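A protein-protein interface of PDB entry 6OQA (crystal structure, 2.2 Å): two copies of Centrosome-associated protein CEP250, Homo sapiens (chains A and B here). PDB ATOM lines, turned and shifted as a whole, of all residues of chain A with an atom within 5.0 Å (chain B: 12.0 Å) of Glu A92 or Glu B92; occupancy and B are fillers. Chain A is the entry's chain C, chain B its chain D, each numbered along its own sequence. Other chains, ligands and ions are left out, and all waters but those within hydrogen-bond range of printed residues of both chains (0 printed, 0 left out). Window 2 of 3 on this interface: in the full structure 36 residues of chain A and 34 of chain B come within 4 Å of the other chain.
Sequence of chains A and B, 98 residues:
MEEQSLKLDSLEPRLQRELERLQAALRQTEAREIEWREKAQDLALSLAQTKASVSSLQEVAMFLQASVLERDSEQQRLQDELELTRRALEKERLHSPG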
ATOM      1  N   ALA A  88      19.936 -14.404  22.998  1.00  0.00           N
ATOM      2  CA  ALA A  88      20.471 -15.092  21.818  1.00  0.00           C
ATOM      3  C   ALA A  88      20.955 -16.504  22.151  1.00  0.00           C
ATOM      4  O   ALA A  88      20.674 -17.438  21.405  1.00  0.00           O
ATOM      5  CB  ALA A  88      21.590 -14.277  21.184  1.00  0.00           C
ATOM      6  N   LEU A  89      21.654 -16.657  23.276  1.00  0.00           N
ATOM      7  CA  LEU A  89      22.112 -17.972  23.741  1.00  0.00           C
ATOM      8  C   LEU A  89      20.934 -18.902  24.047  1.00  0.00           C
ATOM      9  O   LEU A  89      20.937 -20.072  23.652  1.00  0.00           O
ATOM     10  CB  LEU A  89      22.999 -17.829  24.988  1.00  0.00           C
ATOM     11  CG  LEU A  89      23.562 -19.106  25.632  1.00  0.00           C
ATOM     12  CD1 LEU A  89      24.232 -19.989  24.588  1.00  0.00           C
ATOM     13  CD2 LEU A  89      24.539 -18.769  26.751  1.00  0.00           C
ATOM     14  N   GLU A  90      19.937 -18.365  24.746  1.00  0.00           N
ATOM     15  CA  GLU A  90      18.708 -19.100  25.076  1.00  0.00           C
ATOM     16  C   GLU A  90      17.940 -19.564  23.830  1.00  0.00           C
ATOM     17  O   GLU A  90      17.461 -20.697  23.791  1.00  0.00           O
ATOM     18  CB  GLU A  90      17.800 -18.242  25.970  1.00  0.00           C
ATOM     19  CG  GLU A  90      18.349 -18.043  27.382  1.00  0.00           C
ATOM     20  CD  GLU A  90      17.785 -16.826  28.103  1.00  0.00           C
ATOM     21  OE1 GLU A  90      16.745 -16.271  27.679  1.00  0.00           O
ATOM     22  OE2 GLU A  90      18.386 -16.417  29.117  1.00  0.00           O
ATOM     23  N   LYS A  91      17.835 -18.694  22.822  1.00  0.00           N
ATOM     24  CA  LYS A  91      17.177 -19.039  21.552  1.00  0.00           C
ATOM     25  C   LYS A  91      17.924 -20.111  20.745  1.00  0.00           C
ATOM     26  O   LYS A  91      17.286 -20.903  20.051  1.00  0.00           O
ATOM     27  CB  LYS A  91      16.957 -17.800  20.672  1.00  0.00           C
ATOM     28  CG  LYS A  91      15.867 -16.861  21.174  1.00  0.00           C
ATOM     29  CD  LYS A  91      15.223 -16.067  20.044  1.00  0.00           C
ATOM     30  CE  LYS A  91      14.552 -14.789  20.540  1.00  0.00           C
ATOM     31  NZ  LYS A  91      13.231 -14.573  19.887  1.00  0.00           N
ATOM     32  N   GLU A  92      19.258 -20.120  20.821  1.00  0.00           N
ATOM     33  CA  GLU A  92      20.075 -21.180  20.202  1.00  0.00           C
ATOM     34  C   GLU A  92      19.868 -22.545  20.871  1.00  0.00           C
ATOM     35  O   GLU A  92      19.883 -23.575  20.195  1.00  0.00           O
ATOM     36  CB  GLU A  92      21.566 -20.816  20.230  1.00  0.00           C
ATOM     37  CG  GLU A  92      21.950 -19.655  19.317  1.00  0.00           C
ATOM     38  CD  GLU A  92      21.983 -20.005  17.839  1.00  0.00           C
ATOM     39  OE1 GLU A  92      22.206 -21.185  17.489  1.00  0.00           O
ATOM     40  OE2 GLU A  92      21.799 -19.081  17.018  1.00  0.00           O
ATOM     41  N   ARG A  93      19.682 -22.542  22.193  1.00  0.00           N
ATOM     42  CA  ARG A  93      19.385 -23.769  22.952  1.00  0.00           C
ATOM     43  C   ARG A  93      17.944 -24.293  22.786  1.00  0.00           C
ATOM     44  O   ARG A  93      17.659 -25.426  23.184  1.00  0.00           O
ATOM     45  CB  ARG A  93      19.721 -23.574  24.437  1.00  0.00           C
ATOM     46  CG  ARG A  93      21.217 -23.536  24.702  1.00  0.00           C
ATOM     47  CD  ARG A  93      21.547 -23.021  26.091  1.00  0.00           C
ATOM     48  NE  ARG A  93      22.994 -22.985  26.326  1.00  0.00           N
ATOM     49  CZ  ARG A  93      23.594 -22.453  27.395  1.00  0.00           C
ATOM     50  NH1 ARG A  93      22.888 -21.883  28.376  1.00  0.00           N
ATOM     51  NH2 ARG A  93      24.922 -22.486  27.487  1.00  0.00           N
ATOM     52  N   LEU A  94      17.050 -23.481  22.214  1.00  0.00           N
ATOM     53  CA  LEU A  94      15.700 -23.920  21.828  1.00  0.00           C
ATOM     54  C   LEU A  94      15.659 -24.269  20.340  1.00  0.00           C
ATOM     55  O   LEU A  94      15.359 -25.404  19.970  1.00  0.00           O
ATOM     56  CB  LEU A  94      14.657 -22.834  22.132  1.00  0.00           C
ATOM     57  CG  LEU A  94      14.222 -22.680  23.591  1.00  0.00           C
ATOM     58  CD1 LEU A  94      13.519 -21.348  23.803  1.00  0.00           C
ATOM     59  CD2 LEU A  94      13.326 -23.833  24.014  1.00  0.00           C
ATOM     60  N   HIS A  95      15.970 -23.280  19.502  1.00  0.00           N
ATOM     61  CA  HIS A  95      15.881 -23.414  18.043  1.00  0.00           C
ATOM     62  C   HIS A  95      17.171 -23.938  17.483  1.00  0.00           C
ATOM     63  O   HIS A  95      17.223 -25.044  16.942  1.00  0.00           O
ATOM     64  CB  HIS A  95      15.543 -22.070  17.396  1.00  0.00           C
ATOM     65  CG  HIS A  95      14.306 -21.408  17.963  1.00  0.00           C
ATOM     66  ND1 HIS A  95      13.067 -21.892  17.763  1.00  0.00           N
ATOM     67  CD2 HIS A  95      14.157 -20.259  18.740  1.00  0.00           C
ATOM     68  CE1 HIS A  95      12.169 -21.100  18.381  1.00  0.00           C
ATOM     69  NE2 HIS A  95      12.838 -20.100  18.979  1.00  0.00           N
ATOM     70  N   GLU B  83      32.036 -11.324  28.349  1.00  0.00           N
ATOM     71  CA  GLU B  83      33.041 -12.077  27.588  1.00  0.00           C
ATOM     72  C   GLU B  83      32.757 -13.584  27.601  1.00  0.00           C
ATOM     73  O   GLU B  83      32.765 -14.218  26.545  1.00  0.00           O
ATOM     74  CB  GLU B  83      34.468 -11.793  28.094  1.00  0.00           C
ATOM     75  CG  GLU B  83      35.558 -12.336  27.160  1.00  0.00           C
ATOM     76  CD  GLU B  83      36.981 -11.923  27.523  1.00  0.00           C
ATOM     77  OE1 GLU B  83      37.186 -10.935  28.259  1.00  0.00           O
ATOM     78  OE2 GLU B  83      37.921 -12.599  27.055  1.00  0.00           O
ATOM     79  N   LEU B  84      32.488 -14.136  28.786  1.00  0.00           N
ATOM     80  CA  LEU B  84      32.166 -15.566  28.935  1.00  0.00           C
ATOM     81  C   LEU B  84      30.860 -15.950  28.230  1.00  0.00           C
ATOM     82  O   LEU B  84      30.792 -16.989  27.562  1.00  0.00           O
ATOM     83  CB  LEU B  84      32.074 -15.959  30.415  1.00  0.00           C
ATOM     84  CG  LEU B  84      33.369 -15.853  31.226  1.00  0.00           C
ATOM     85  CD1 LEU B  84      33.080 -16.011  32.708  1.00  0.00           C
ATOM     86  CD2 LEU B  84      34.401 -16.875  30.770  1.00  0.00           C
ATOM     87  N   THR B  85      29.836 -15.112  28.377  1.00  0.00           N
ATOM     88  CA  THR B  85      28.543 -15.350  27.732  1.00  0.00           C
ATOM     89  C   THR B  85      28.648 -15.280  26.202  1.00  0.00           C
ATOM     90  O   THR B  85      27.993 -16.059  25.516  1.00  0.00           O
ATOM     91  CB  THR B  85      27.461 -14.371  28.233  1.00  0.00           C
ATOM     92  OG1 THR B  85      27.459 -14.356  29.662  1.00  0.00           O
ATOM     93  CG2 THR B  85      26.077 -14.792  27.751  1.00  0.00           C
ATOM     94  N   ARG B  86      29.459 -14.354  25.680  1.00  0.00           N
ATOM     95  CA  ARG B  86      29.752 -14.298  24.234  1.00  0.00           C
ATOM     96  C   ARG B  86      30.478 -15.563  23.761  1.00  0.00           C
ATOM     97  O   ARG B  86      30.171 -16.094  22.694  1.00  0.00           O
ATOM     98  CB  ARG B  86      30.577 -13.053  23.853  1.00  0.00           C
ATOM     99  CG  ARG B  86      29.751 -11.790  23.653  1.00  0.00           C
ATOM    100  CD  ARG B  86      30.477 -10.700  22.865  1.00  0.00           C
ATOM    101  NE  ARG B  86      31.134  -9.701  23.724  1.00  0.00           N
ATOM    102  CZ  ARG B  86      32.451  -9.552  23.926  1.00  0.00           C
ATOM    103  NH1 ARG B  86      33.360 -10.338  23.336  1.00  0.00           N
ATOM    104  NH2 ARG B  86      32.876  -8.584  24.741  1.00  0.00           N
ATOM    105  N   ARG B  87      31.430 -16.034  24.562  1.00  0.00           N
ATOM    106  CA  ARG B  87      32.190 -17.247  24.248  1.00  0.00           C
ATOM    107  C   ARG B  87      31.269 -18.466  24.174  1.00  0.00           C
ATOM    108  O   ARG B  87      31.318 -19.220  23.198  1.00  0.00           O
ATOM    109  CB  ARG B  87      33.302 -17.475  25.282  1.00  0.00           C
ATOM    110  CG  ARG B  87      34.381 -18.455  24.843  1.00  0.00           C
ATOM    111  CD  ARG B  87      35.678 -18.255  25.620  1.00  0.00           C
ATOM    112  NE  ARG B  87      35.558 -18.641  27.028  1.00  0.00           N
ATOM    113  CZ  ARG B  87      36.493 -18.447  27.964  1.00  0.00           C
ATOM    114  NH1 ARG B  87      37.656 -17.859  27.677  1.00  0.00           N
ATOM    115  NH2 ARG B  87      36.263 -18.851  29.213  1.00  0.00           N
ATOM    116  N   ALA B  88      30.418 -18.625  25.191  1.00  0.00           N
ATOM    117  CA  ALA B  88      29.406 -19.696  25.218  1.00  0.00           C
ATOM    118  C   ALA B  88      28.442 -19.660  24.017  1.00  0.00           C
ATOM    119  O   ALA B  88      28.079 -20.716  23.495  1.00  0.00           O
ATOM    120  CB  ALA B  88      28.623 -19.663  26.528  1.00  0.00           C
ATOM    121  N   LEU B  89      28.048 -18.459  23.579  1.00  0.00           N
ATOM    122  CA  LEU B  89      27.188 -18.298  22.394  1.00  0.00           C
ATOM    123  C   LEU B  89      27.882 -18.748  21.104  1.00  0.00           C
ATOM    124  O   LEU B  89      27.246 -19.366  20.251  1.00  0.00           O
ATOM    125  CB  LEU B  89      26.708 -16.848  22.239  1.00  0.00           C
ATOM    126  CG  LEU B  89      25.857 -16.502  21.006  1.00  0.00           C
ATOM    127  CD1 LEU B  89      24.616 -17.384  20.929  1.00  0.00           C
ATOM    128  CD2 LEU B  89      25.465 -15.033  21.013  1.00  0.00           C
ATOM    129  N   GLU B  90      29.165 -18.415  20.959  1.00  0.00           N
ATOM    130  CA  GLU B  90      29.968 -18.882  19.815  1.00  0.00           C
ATOM    131  C   GLU B  90      30.157 -20.402  19.812  1.00  0.00           C
ATOM    132  O   GLU B  90      30.099 -21.024  18.753  1.00  0.00           O
ATOM    133  CB  GLU B  90      31.339 -18.188  19.767  1.00  0.00           C
ATOM    134  CG  GLU B  90      31.314 -16.792  19.148  1.00  0.00           C
ATOM    135  CD  GLU B  90      32.637 -16.395  18.506  1.00  0.00           C
ATOM    136  OE1 GLU B  90      33.171 -17.180  17.689  1.00  0.00           O
ATOM    137  OE2 GLU B  90      33.138 -15.289  18.804  1.00  0.00           O
ATOM    138  N   LYS B  91      30.391 -20.985  20.988  1.00  0.00           N
ATOM    139  CA  LYS B  91      30.500 -22.446  21.135  1.00  0.00           C
ATOM    140  C   LYS B  91      29.211 -23.172  20.736  1.00  0.00           C
ATOM    141  O   LYS B  91      29.265 -24.232  20.112  1.00  0.00           O
ATOM    142  CB  LYS B  91      30.883 -22.838  22.571  1.00  0.00           C
ATOM    143  CG  LYS B  91      32.358 -22.674  22.897  1.00  0.00           C
ATOM    144  CD  LYS B  91      32.663 -23.165  24.306  1.00  0.00           C
ATOM    145  CE  LYS B  91      34.096 -22.862  24.715  1.00  0.00           C
ATOM    146  NZ  LYS B  91      34.315 -23.046  26.178  1.00  0.00           N
ATOM    147  N   GLU B  92      28.068 -22.595  21.102  1.00  0.00           N
ATOM    148  CA  GLU B  92      26.756 -23.153  20.757  1.00  0.00           C
ATOM    149  C   GLU B  92      26.446 -23.025  19.256  1.00  0.00           C
ATOM    150  O   GLU B  92      25.869 -23.939  18.664  1.00  0.00           O
ATOM    151  CB  GLU B  92      25.651 -22.479  21.585  1.00  0.00           C
ATOM    152  CG  GLU B  92      24.337 -23.251  21.649  1.00  0.00           C
ATOM    153  CD  GLU B  92      24.430 -24.546  22.442  1.00  0.00           C
ATOM    154  OE1 GLU B  92      25.083 -24.557  23.508  1.00  0.00           O
ATOM    155  OE2 GLU B  92      23.836 -25.554  22.002  1.00  0.00           O
ATOM    156  N   ARG B  93      26.829 -21.897  18.656  1.00  0.00           N
ATOM    157  CA  ARG B  93      26.621 -21.662  17.216  1.00  0.00           C
ATOM    158  C   ARG B  93      27.447 -22.577  16.295  1.00  0.00           C
ATOM    159  O   ARG B  93      27.052 -22.799  15.148  1.00  0.00           O
ATOM    160  CB  ARG B  93      26.862 -20.189  16.860  1.00  0.00           C
ATOM    161  CG  ARG B  93      25.710 -19.284  17.268  1.00  0.00           C
ATOM    162  CD  ARG B  93      26.040 -17.812  17.087  1.00  0.00           C
ATOM    163  NE  ARG B  93      24.882 -16.965  17.382  1.00  0.00           N
ATOM    164  CZ  ARG B  93      24.884 -15.630  17.394  1.00  0.00           C
ATOM    165  NH1 ARG B  93      25.995 -14.938  17.128  1.00  0.00           N
ATOM    166  NH2 ARG B  93      23.760 -14.975  17.677  1.00  0.00           N
ATOM    167  N   LEU B  94      28.578 -23.093  16.787  1.00  0.00           N
ATOM    168  CA  LEU B  94      29.347 -24.122  16.068  1.00  0.00           C
ATOM    169  C   LEU B  94      28.602 -25.455  16.101  1.00  0.00           C
ATOM    170  O   LEU B  94      28.286 -26.025  15.055  1.00  0.00           O
ATOM    171  CB  LEU B  94      30.746 -24.306  16.676  1.00  0.00           C
ATOM    172  CG  LEU B  94      31.768 -23.188  16.464  1.00  0.00           C
ATOM    173  CD1 LEU B  94      33.015 -23.463  17.291  1.00  0.00           C
ATOM    174  CD2 LEU B  94      32.131 -23.032  14.995  1.00  0.00           C
ATOM    175  N   HIS B  95      28.326 -25.934  17.312  1.00  0.00           N
ATOM    176  CA  HIS B  95      27.606 -27.191  17.519  1.00  0.00           C
ATOM    177  C   HIS B  95      26.128 -26.970  17.377  1.00  0.00           C
ATOM    178  O   HIS B  95      25.352 -27.921  17.296  1.00  0.00           O
ATOM    179  CB  HIS B  95      27.919 -27.767  18.896  1.00  0.00           C
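Ala A88 touches Leu B89.
Leu B89 touches Leu A89.
Glu A92 touches Leu B89.
Glu A92 touches Glu B92.
Ala A88 touches Leu B89, but with the chains exchanged Leu A89 does not touch Ala B88 (4.1 Å).
Leu A89 touches its own counterpart, Leu B89.
Glu A92 touches Leu B89, but with the chains exchanged Leu A89 does not touch Glu B92 (4.2 Å).
Glu A92 touches Arg B93, and with the chains exchanged Arg A93 touches Glu B92.
Positions printed for both chains: 88, 89, 90, 91, 92, 93, 94 and 95.
Of the 6 pairs that touch across the chains among the printed residues, 4 have their exchanged pair printed and touching as well.
OE2 of Glu A92 is in salt-bridge range of NE of Arg B93, 3.8 Å away.
The guanidinium group (NE) of Arg A93 is in salt-bridge range of the side-chain carboxylate (OE1) of Glu B92, at 3.8 Å.
Printed residues of chain A within 4 Å of Glu B92: Glu A92 and Arg A93.
Ala A88 touches just one residue of chain B: Leu B89.
Leu A89 touches just one residue of chain B: Leu B89.
Of chain B, only Glu B92 comes within 4 Å of Arg A93.
Leu A94 touches none of the printed residues of chain B.
No residue of chain B comes within 4 Å of His A95.
Of the printed residues of chain A, Leu B89 touches Ala A88, Leu A89 and Glu A92.
Printed residues of chain A within 4 Å of Arg B93: Glu A92.
Lys B91 touches none of the printed residues of chain A.
The nearest residue of chain A that does not touch Glu B92 is Leu A89 (4.2 Å).
Of the 8 printed residues of chain A, 4 touch a printed residue of chain B.
Printed residues of chain A that touch a printed residue of chain B: Ala A88, Leu A89, Glu A92 and Arg A93.
Hydrophobic or aromatic side chains of chain A within 4 Å of the printed part of chain B: Ala A88.
Printed residues of chain B that touch a printed residue of chain A: Leu B89, Glu B92 and Arg B93.
Hydrophobic or aromatic side chains of chain B that line the printed part of chain A: Leu B89.
Among the printed residues, 6 pairs touch across the chains.
Among the printed residues, Asp or Glu carboxylates within 4 Å of a Lys or Arg side-chain nitrogen of the other chain: Glu A92 with Arg B93 and Arg A93 with Glu B92.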
